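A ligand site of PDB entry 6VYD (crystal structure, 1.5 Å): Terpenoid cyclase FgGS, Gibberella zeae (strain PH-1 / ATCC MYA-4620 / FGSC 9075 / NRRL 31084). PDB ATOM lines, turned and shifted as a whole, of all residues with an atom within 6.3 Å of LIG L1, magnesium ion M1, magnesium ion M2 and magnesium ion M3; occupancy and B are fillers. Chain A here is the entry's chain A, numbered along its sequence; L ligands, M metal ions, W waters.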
ATOM      1  N   PHE A  91     -27.431 -15.985  -8.779  1.00  0.00           N
ATOM      2  CA  PHE A  91     -27.015 -15.602 -10.130  1.00  0.00           C
ATOM      3  C   PHE A  91     -25.769 -14.719 -10.084  1.00  0.00           C
ATOM      4  O   PHE A  91     -24.870 -14.848 -10.933  1.00  0.00           O
ATOM      5  CB  PHE A  91     -28.130 -14.789 -10.793  1.00  0.00           C
ATOM      6  CG  PHE A  91     -29.113 -15.596 -11.595  1.00  0.00           C
ATOM      7  CD1 PHE A  91     -28.764 -16.198 -12.794  1.00  0.00           C
ATOM      8  CD2 PHE A  91     -30.449 -15.666 -11.177  1.00  0.00           C
ATOM      9  CE1 PHE A  91     -29.709 -16.887 -13.545  1.00  0.00           C
ATOM     10  CE2 PHE A  91     -31.381 -16.369 -11.901  1.00  0.00           C
ATOM     11  CZ  PHE A  91     -31.042 -16.980 -13.081  1.00  0.00           C
ATOM     12  N   ASP A  94     -22.696 -16.593  -8.680  1.00  0.00           N
ATOM     13  CA  ASP A  94     -22.220 -17.535  -9.691  1.00  0.00           C
ATOM     14  C   ASP A  94     -21.103 -16.914 -10.532  1.00  0.00           C
ATOM     15  O   ASP A  94     -20.046 -17.530 -10.769  1.00  0.00           O
ATOM     16  CB  ASP A  94     -23.427 -17.911 -10.576  1.00  0.00           C
ATOM     17  CG  ASP A  94     -23.005 -18.615 -11.848  1.00  0.00           C
ATOM     18  OD1 ASP A  94     -22.500 -19.766 -11.746  1.00  0.00           O
ATOM     19  OD2 ASP A  94     -23.116 -17.998 -12.931  1.00  0.00           O
ATOM     20  N   SER A  95     -21.320 -15.691 -11.010  1.00  0.00           N
ATOM     21  CA  SER A  95     -20.298 -15.075 -11.853  1.00  0.00           C
ATOM     22  C   SER A  95     -19.019 -14.779 -11.070  1.00  0.00           C
ATOM     23  O   SER A  95     -17.920 -14.835 -11.629  1.00  0.00           O
ATOM     24  CB  SER A  95     -20.897 -13.830 -12.535  1.00  0.00           C
ATOM     25  OG  SER A  95     -22.034 -14.224 -13.283  1.00  0.00           O
ATOM     26  N   GLU A  98     -17.038 -18.017 -11.033  1.00  0.00           N
ATOM     27  CA  GLU A  98     -16.412 -18.337 -12.305  1.00  0.00           C
ATOM     28  C   GLU A  98     -15.325 -17.338 -12.682  1.00  0.00           C
ATOM     29  O   GLU A  98     -14.504 -17.625 -13.572  1.00  0.00           O
ATOM     30  CB  GLU A  98     -17.474 -18.357 -13.417  1.00  0.00           C
ATOM     31  CG  GLU A  98     -18.534 -19.470 -13.353  1.00  0.00           C
ATOM     32  CD  GLU A  98     -19.581 -19.311 -14.445  1.00  0.00           C
ATOM     33  OE1 GLU A  98     -19.194 -19.045 -15.622  1.00  0.00           O
ATOM     34  OE2 GLU A  98     -20.783 -19.438 -14.130  1.00  0.00           O
ATOM     35  N   THR A 147     -18.219 -26.118  -7.656  1.00  0.00           N
ATOM     36  CA  THR A 147     -17.688 -25.135  -8.609  1.00  0.00           C
ATOM     37  C   THR A 147     -16.271 -24.727  -8.244  1.00  0.00           C
ATOM     38  O   THR A 147     -15.371 -24.720  -9.095  1.00  0.00           O
ATOM     39  CB  THR A 147     -18.593 -23.898  -8.616  1.00  0.00           C
ATOM     40  OG1 THR A 147     -19.899 -24.296  -9.068  1.00  0.00           O
ATOM     41  CG2 THR A 147     -18.010 -22.866  -9.562  1.00  0.00           C
ATOM     42  N   ARG A 165     -21.549 -30.776 -14.022  1.00  0.00           N
ATOM     43  CA  ARG A 165     -22.330 -29.601 -14.421  1.00  0.00           C
ATOM     44  C   ARG A 165     -23.698 -29.556 -13.742  1.00  0.00           C
ATOM     45  O   ARG A 165     -24.196 -28.454 -13.462  1.00  0.00           O
ATOM     46  CB  ARG A 165     -22.502 -29.610 -15.936  1.00  0.00           C
ATOM     47  CG  ARG A 165     -23.091 -28.311 -16.519  1.00  0.00           C
ATOM     48  CD  ARG A 165     -22.209 -27.067 -16.318  1.00  0.00           C
ATOM     49  NE  ARG A 165     -22.880 -26.028 -17.091  1.00  0.00           N
ATOM     50  CZ  ARG A 165     -23.469 -24.968 -16.571  1.00  0.00           C
ATOM     51  NH1 ARG A 165     -23.283 -24.642 -15.270  1.00  0.00           N
ATOM     52  NH2 ARG A 165     -24.277 -24.254 -17.360  1.00  0.00           N
ATOM     53  N   ASP A 168     -22.774 -27.896 -10.551  1.00  0.00           N
ATOM     54  CA  ASP A 168     -22.258 -26.549 -10.781  1.00  0.00           C
ATOM     55  C   ASP A 168     -23.386 -25.585 -11.155  1.00  0.00           C
ATOM     56  O   ASP A 168     -23.393 -24.417 -10.715  1.00  0.00           O
ATOM     57  CB  ASP A 168     -21.215 -26.606 -11.909  1.00  0.00           C
ATOM     58  CG  ASP A 168     -20.779 -25.223 -12.437  1.00  0.00           C
ATOM     59  OD1 ASP A 168     -21.012 -24.946 -13.632  1.00  0.00           O
ATOM     60  OD2 ASP A 168     -20.135 -24.481 -11.684  1.00  0.00           O
ATOM     61  N   THR A 169     -24.341 -26.037 -11.980  1.00  0.00           N
ATOM     62  CA  THR A 169     -25.442 -25.141 -12.353  1.00  0.00           C
ATOM     63  C   THR A 169     -26.463 -25.009 -11.231  1.00  0.00           C
ATOM     64  O   THR A 169     -27.366 -24.176 -11.312  1.00  0.00           O
ATOM     65  CB  THR A 169     -26.071 -25.595 -13.693  1.00  0.00           C
ATOM     66  OG1 THR A 169     -26.720 -24.493 -14.368  1.00  0.00           O
ATOM     67  CG2 THR A 169     -27.080 -26.735 -13.484  1.00  0.00           C
ATOM     68  N   GLY A 170     -26.326 -25.801 -10.166  1.00  0.00           N
ATOM     69  CA  GLY A 170     -27.259 -25.694  -9.054  1.00  0.00           C
ATOM     70  C   GLY A 170     -28.604 -26.333  -9.304  1.00  0.00           C
ATOM     71  O   GLY A 170     -29.621 -25.873  -8.744  1.00  0.00           O
ATOM     72  N   ALA A 206     -29.181 -28.070 -17.686  1.00  0.00           N
ATOM     73  CA  ALA A 206     -27.802 -27.557 -17.772  1.00  0.00           C
ATOM     74  C   ALA A 206     -27.406 -27.345 -19.224  1.00  0.00           C
ATOM     75  O   ALA A 206     -26.836 -26.301 -19.570  1.00  0.00           O
ATOM     76  CB  ALA A 206     -26.848 -28.569 -17.115  1.00  0.00           C
ATOM     77  N   ASN A 209     -29.168 -24.333 -20.676  1.00  0.00           N
ATOM     78  CA  ASN A 209     -28.423 -23.158 -20.276  1.00  0.00           C
ATOM     79  C   ASN A 209     -27.180 -22.969 -21.146  1.00  0.00           C
ATOM     80  O   ASN A 209     -26.905 -21.859 -21.618  1.00  0.00           O
ATOM     81  CB  ASN A 209     -28.045 -23.176 -18.806  1.00  0.00           C
ATOM     82  CG  ASN A 209     -27.188 -21.991 -18.476  1.00  0.00           C
ATOM     83  OD1 ASN A 209     -25.956 -22.067 -18.596  1.00  0.00           O
ATOM     84  ND2 ASN A 209     -27.825 -20.844 -18.164  1.00  0.00           N
ATOM     85  N   ASP A 210     -26.391 -24.043 -21.333  1.00  0.00           N
ATOM     86  CA  ASP A 210     -25.184 -23.919 -22.148  1.00  0.00           C
ATOM     87  C   ASP A 210     -25.516 -23.383 -23.530  1.00  0.00           C
ATOM     88  O   ASP A 210     -24.811 -22.508 -24.045  1.00  0.00           O
ATOM     89  CB  ASP A 210     -24.525 -25.296 -22.311  1.00  0.00           C
ATOM     90  CG  ASP A 210     -23.853 -25.810 -21.056  1.00  0.00           C
ATOM     91  OD1 ASP A 210     -23.462 -26.978 -21.088  1.00  0.00           O
ATOM     92  OD2 ASP A 210     -23.702 -25.077 -20.073  1.00  0.00           O
ATOM     93  N   SER A 213     -26.575 -19.557 -23.275  1.00  0.00           N
ATOM     94  CA  SER A 213     -25.619 -18.663 -22.625  1.00  0.00           C
ATOM     95  C   SER A 213     -24.205 -18.747 -23.229  1.00  0.00           C
ATOM     96  O   SER A 213     -23.340 -17.978 -22.799  1.00  0.00           O
ATOM     97  CB  SER A 213     -25.564 -18.918 -21.110  1.00  0.00           C
ATOM     98  OG  SER A 213     -25.070 -20.236 -20.762  1.00  0.00           O
ATOM     99  N   PHE A 214     -23.983 -19.624 -24.195  1.00  0.00           N
ATOM    100  CA  PHE A 214     -22.673 -19.764 -24.835  1.00  0.00           C
ATOM    101  C   PHE A 214     -22.129 -18.438 -25.358  1.00  0.00           C
ATOM    102  O   PHE A 214     -20.968 -18.095 -25.114  1.00  0.00           O
ATOM    103  CB  PHE A 214     -22.732 -20.793 -25.968  1.00  0.00           C
ATOM    104  CG  PHE A 214     -21.462 -20.919 -26.744  1.00  0.00           C
ATOM    105  CD1 PHE A 214     -20.441 -21.763 -26.315  1.00  0.00           C
ATOM    106  CD2 PHE A 214     -21.277 -20.195 -27.912  1.00  0.00           C
ATOM    107  CE1 PHE A 214     -19.242 -21.872 -27.031  1.00  0.00           C
ATOM    108  CE2 PHE A 214     -20.086 -20.283 -28.632  1.00  0.00           C
ATOM    109  CZ  PHE A 214     -19.083 -21.137 -28.197  1.00  0.00           C
ATOM    110  N   ARG A 216     -22.677 -15.353 -24.656  1.00  0.00           N
ATOM    111  CA  ARG A 216     -22.304 -14.467 -23.558  1.00  0.00           C
ATOM    112  C   ARG A 216     -21.065 -14.994 -22.837  1.00  0.00           C
ATOM    113  O   ARG A 216     -20.202 -14.211 -22.407  1.00  0.00           O
ATOM    114  CB  ARG A 216     -23.541 -14.321 -22.635  1.00  0.00           C
ATOM    115  CG  ARG A 216     -23.290 -13.702 -21.282  1.00  0.00           C
ATOM    116  CD  ARG A 216     -23.119 -14.760 -20.244  1.00  0.00           C
ATOM    117  NE  ARG A 216     -23.197 -14.249 -18.889  1.00  0.00           N
ATOM    118  CZ  ARG A 216     -23.375 -15.039 -17.833  1.00  0.00           C
ATOM    119  NH1 ARG A 216     -23.435 -16.361 -18.026  1.00  0.00           N
ATOM    120  NH2 ARG A 216     -23.439 -14.536 -16.602  1.00  0.00           N
ATOM    121  N   GLU A 217     -20.977 -16.316 -22.662  1.00  0.00           N
ATOM    122  CA  GLU A 217     -19.822 -16.875 -21.950  1.00  0.00           C
ATOM    123  C   GLU A 217     -18.524 -16.775 -22.758  1.00  0.00           C
ATOM    124  O   GLU A 217     -17.428 -16.680 -22.176  1.00  0.00           O
ATOM    125  CB  GLU A 217     -20.124 -18.283 -21.442  1.00  0.00           C
ATOM    126  CG  GLU A 217     -21.267 -18.235 -20.414  1.00  0.00           C
ATOM    127  CD  GLU A 217     -21.806 -19.578 -19.996  1.00  0.00           C
ATOM    128  OE1 GLU A 217     -22.702 -19.564 -19.105  1.00  0.00           O
ATOM    129  OE2 GLU A 217     -21.332 -20.630 -20.539  1.00  0.00           O
ATOM    130  N   ILE A 227     -17.364 -22.802 -18.902  1.00  0.00           N
ATOM    131  CA  ILE A 227     -17.972 -24.081 -18.505  1.00  0.00           C
ATOM    132  C   ILE A 227     -19.177 -24.256 -19.426  1.00  0.00           C
ATOM    133  O   ILE A 227     -20.260 -23.708 -19.170  1.00  0.00           O
ATOM    134  CB  ILE A 227     -18.362 -24.101 -17.026  1.00  0.00           C
ATOM    135  CG1 ILE A 227     -17.155 -23.804 -16.125  1.00  0.00           C
ATOM    136  CG2 ILE A 227     -19.102 -25.383 -16.627  1.00  0.00           C
ATOM    137  CD1 ILE A 227     -17.499 -23.403 -14.682  1.00  0.00           C
ATOM    138  N   ASN A 228     -19.003 -24.991 -20.529  1.00  0.00           N
ATOM    139  CA  ASN A 228     -20.057 -24.987 -21.519  1.00  0.00           C
ATOM    140  C   ASN A 228     -19.873 -26.140 -22.505  1.00  0.00           C
ATOM    141  O   ASN A 228     -18.814 -26.247 -23.166  1.00  0.00           O
ATOM    142  CB  ASN A 228     -20.072 -23.634 -22.264  1.00  0.00           C
ATOM    143  CG  ASN A 228     -21.356 -23.430 -23.081  1.00  0.00           C
ATOM    144  OD1 ASN A 228     -21.689 -24.263 -23.955  1.00  0.00           O
ATOM    145  ND2 ASN A 228     -22.120 -22.373 -22.747  1.00  0.00           N
ATOM    146  N   TRP A 294     -37.446 -18.487 -20.630  1.00  0.00           N
ATOM    147  CA  TRP A 294     -36.717 -17.364 -20.045  1.00  0.00           C
ATOM    148  C   TRP A 294     -35.403 -17.114 -20.776  1.00  0.00           C
ATOM    149  O   TRP A 294     -35.028 -15.957 -21.019  1.00  0.00           O
ATOM    150  CB  TRP A 294     -36.469 -17.664 -18.562  1.00  0.00           C
ATOM    151  CG  TRP A 294     -35.548 -16.697 -17.878  1.00  0.00           C
ATOM    152  CD1 TRP A 294     -35.871 -15.490 -17.318  1.00  0.00           C
ATOM    153  CD2 TRP A 294     -34.131 -16.883 -17.654  1.00  0.00           C
ATOM    154  NE1 TRP A 294     -34.745 -14.906 -16.762  1.00  0.00           N
ATOM    155  CE2 TRP A 294     -33.664 -15.734 -16.966  1.00  0.00           C
ATOM    156  CE3 TRP A 294     -33.214 -17.892 -17.974  1.00  0.00           C
ATOM    157  CZ2 TRP A 294     -32.318 -15.578 -16.576  1.00  0.00           C
ATOM    158  CZ3 TRP A 294     -31.882 -17.753 -17.571  1.00  0.00           C
ATOM    159  CH2 TRP A 294     -31.447 -16.600 -16.903  1.00  0.00           C
ATOM    160  N   ARG A 300     -29.676 -11.300 -19.227  1.00  0.00           N
ATOM    161  CA  ARG A 300     -28.387 -11.880 -18.825  1.00  0.00           C
ATOM    162  C   ARG A 300     -27.627 -12.421 -20.018  1.00  0.00           C
ATOM    163  O   ARG A 300     -26.399 -12.279 -20.086  1.00  0.00           O
ATOM    164  CB  ARG A 300     -28.638 -12.972 -17.787  1.00  0.00           C
ATOM    165  CG  ARG A 300     -27.337 -13.552 -17.142  1.00  0.00           C
ATOM    166  CD  ARG A 300     -27.769 -14.507 -16.024  1.00  0.00           C
ATOM    167  NE  ARG A 300     -26.690 -15.293 -15.426  1.00  0.00           N
ATOM    168  CZ  ARG A 300     -25.948 -14.869 -14.406  1.00  0.00           C
ATOM    169  NH1 ARG A 300     -26.156 -13.644 -13.909  1.00  0.00           N
ATOM    170  NH2 ARG A 300     -24.972 -15.637 -13.907  1.00  0.00           N
ATOM    171  N   TYR A 301     -28.316 -13.069 -20.973  1.00  0.00           N
ATOM    172  CA  TYR A 301     -27.611 -13.706 -22.093  1.00  0.00           C
ATOM    173  C   TYR A 301     -27.726 -12.945 -23.398  1.00  0.00           C
ATOM    174  O   TYR A 301     -26.992 -13.242 -24.344  1.00  0.00           O
ATOM    175  CB  TYR A 301     -28.093 -15.129 -22.391  1.00  0.00           C
ATOM    176  CG  TYR A 301     -28.183 -15.993 -21.154  1.00  0.00           C
ATOM    177  CD1 TYR A 301     -27.298 -15.816 -20.079  1.00  0.00           C
ATOM    178  CD2 TYR A 301     -29.196 -16.951 -21.039  1.00  0.00           C
ATOM    179  CE1 TYR A 301     -27.424 -16.595 -18.929  1.00  0.00           C
ATOM    180  CE2 TYR A 301     -29.322 -17.731 -19.890  1.00  0.00           C
ATOM    181  CZ  TYR A 301     -28.460 -17.528 -18.835  1.00  0.00           C
ATOM    182  OH  TYR A 301     -28.620 -18.275 -17.704  1.00  0.00           O
HETATM  183  P1  LIG L   1     -24.251 -21.152 -15.433  1.00  0.00           P
HETATM  184  O1  LIG L   1     -23.811 -21.363 -16.852  1.00  0.00           O
HETATM  185  O2  LIG L   1     -23.236 -20.385 -14.618  1.00  0.00           O
HETATM  186  O3  LIG L   1     -24.803 -22.356 -14.744  1.00  0.00           O
HETATM  187  O4  LIG L   1     -25.505 -20.103 -15.461  1.00  0.00           O
HETATM  188  P2  LIG L   1     -25.449 -18.729 -16.335  1.00  0.00           P
HETATM  189  O5  LIG L   1     -26.734 -17.996 -16.013  1.00  0.00           O
HETATM  190  O6  LIG L   1     -24.252 -17.976 -15.834  1.00  0.00           O
HETATM  191  O7  LIG L   1     -25.329 -19.096 -17.766  1.00  0.00           O
HETATM  192  N1  LG2 L   2     -29.072 -21.288 -12.906  1.00  0.00           N
HETATM  193  C1  LG2 L   2     -29.121 -22.724 -13.613  1.00  0.00           C
HETATM  194  C2  LG2 L   2     -29.661 -21.346 -11.478  1.00  0.00           C
HETATM  195  C3  LG2 L   2     -29.649 -20.009 -10.739  1.00  0.00           C
HETATM  196  C4  LG2 L   2     -27.503 -20.925 -12.864  1.00  0.00           C
HETATM  197  C5  LG2 L   2     -27.151 -19.470 -12.755  1.00  0.00           C
HETATM  198  C6  LG2 L   2     -29.936 -20.223 -13.710  1.00  0.00           C
HETATM  199  C7  LG2 L   2     -29.547 -20.189 -15.188  1.00  0.00           C
HETATM  200  C8  LG2 L   2     -30.424 -23.427 -13.521  1.00  0.00           C
HETATM  201  C9  LG2 L   2     -30.682 -24.375 -12.525  1.00  0.00           C
HETATM  202  C10 LG2 L   2     -31.927 -25.011 -12.507  1.00  0.00           C
HETATM  203  C11 LG2 L   2     -32.916 -24.736 -13.434  1.00  0.00           C
HETATM  204  C12 LG2 L   2     -32.630 -23.861 -14.458  1.00  0.00           C
HETATM  205  C13 LG2 L   2     -31.400 -23.220 -14.492  1.00  0.00           C
HETATM  206 MG    MG M   1     -22.536 -18.506 -14.888  1.00  0.00          MG
HETATM  207 MG    MG M   2     -21.766 -21.057 -13.215  1.00  0.00          MG
HETATM  208 MG    MG M   3     -24.375 -20.700 -18.660  1.00  0.00          MG
HETATM  209  O   HOH W   1     -20.862 -22.347 -14.474  1.00  0.00           O
HETATM  210  O   HOH W   2     -21.157 -22.001 -17.182  1.00  0.00           O
HETATM  211  O   HOH W   3     -20.382 -21.763 -11.764  1.00  0.00           O
HETATM  212  O   HOH W   4     -21.754 -16.464 -14.821  1.00  0.00           O
HETATM  213  O   HOH W   5     -21.611 -18.650 -16.767  1.00  0.00           O
HETATM  214  O   HOH W   6     -23.344 -22.307 -19.603  1.00  0.00           O
HETATM  215  O   HOH W   7     -23.211 -22.392 -12.531  1.00  0.00           O
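O5 of LIG L1 lies within hydrogen-bond range of OH of Tyr 301, 2.5 Å away.
The guanidinium group of Arg 300 is in salt-bridge range of an oxygen (O5) of LIG L1 (2.8 Å).
An oxygen (O3) of LIG L1 is in salt-bridge range of the guanidinium group (NH1) of Arg 165 (2.8 Å).
O6 of LIG L1 sits close to NH1 of Arg 216 (2.8 Å).
O3 of LIG L1 sits at hydrogen-bond distance from OG1 of Thr 169 (2.9 Å).
Water W5 lies within hydrogen-bond range of OE1 of Glu 98 (2.7 Å) and NH1 of Arg 216 (3.2 Å).
Water W4 lies within hydrogen-bond range of OG of Ser 95 (2.7 Å), NH2 of Arg 216 (3.1 Å) and NH2 of Arg 300 (3.4 Å).
Water W7 lies within hydrogen-bond range of an oxygen (O3) of LIG L1 (2.7 Å) and the backbone carbonyl oxygen of Asp 168 (2.7 Å).
Water W1 lies within hydrogen-bond range of the side-chain carboxylate of Asp 168 (2.7 Å) and the guanidinium group of Arg 165 (3.4 Å).
OE1 of Glu 217 sits close to NH1 of Arg 216 (3.5 Å).
OE2 of Glu 217 sits at hydrogen-bond distance from ND2 of Asn 228.
OD2 of Asp 94 sits close to NH2 of Arg 300, 3.2 Å away.
The side-chain amide nitrogen of Asn 209 is in hydrogen-bond range of the side-chain hydroxyl of Tyr 301 (2.7 Å).
The guanidinium group of Arg 300 sits at hydrogen-bond distance from the backbone carbonyl oxygen of Phe 91, at 3.1 Å.
NH1 of Arg 165 is in salt-bridge range of OD1 of Asp 168, 2.8 Å away.
The guanidinium group of Arg 165 is in salt-bridge range of the side-chain carboxylate of Asp 210 (2.9 Å).
The side-chain carboxylate of Asp 168 is in hydrogen-bond range of the side-chain hydroxyl of Thr 147, 2.6 Å away.
Residues that only touch magnesium ion M2: Asp 168.
Of the 21 residues printed, 3 come within 4 Å of magnesium ion M2.
Magnesium ion M1 is bound by an oxygen (O2) of LIG L1 (2.0 Å), an oxygen (O6) of LIG L1 (2.0 Å), water W5 (2.1 Å), the side-chain carboxylate of Asp 94 (2.1 Å), the side-chain carboxylate of Glu 98 (2.1 Å) and water W4 (2.2 Å).
Magnesium ion M1 has six donor atoms within binding distance.
Arg 165 touches magnesium ion M3 (NH2 to MG, 3.8 Å).
Of the 21 residues printed, 4 come within 4 Å of magnesium ion M3.
The nearest printed residue that does not touch magnesium ion M3 is Arg 216 (4.5 Å).
Magnesium ion M3 is bound by an oxygen (O1) of LIG L1 (2.0 Å), an oxygen (O7) of LIG L1 (2.1 Å), the side-chain carboxylate of Glu 217 (2.1 Å), the side-chain amide oxygen of Asn 209 (2.1 Å), water W6 (2.1 Å) and the side-chain hydroxyl of Ser 213 (2.3 Å).
Water W1 binds magnesium ion M2 (2.0 Å).
Magnesium ion M2 is bound by water W7, at 2.1 Å.
The side-chain carboxylate (OD1) of Asp 94 binds magnesium ion M2 (2.1 Å).
OE2 of Glu 98 binds magnesium ion M2 (2.1 Å).
Water W3 binds magnesium ion M2 (2.1 Å).
Magnesium ion M2 is bound by O2 of LIG L1.
Merely in contact with magnesium ion M1: Arg 300 (3.9 Å) and Arg 216 (3.9 Å).
Along chain A the residues within 4 Å of magnesium ion M1 span positions 94 to 300.
The nearest printed residue that does not touch magnesium ion M1 is Glu 217 (4.4 Å).
Hydrophobic or aromatic side chains within 4 Å of LIG L1: Tyr 301.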
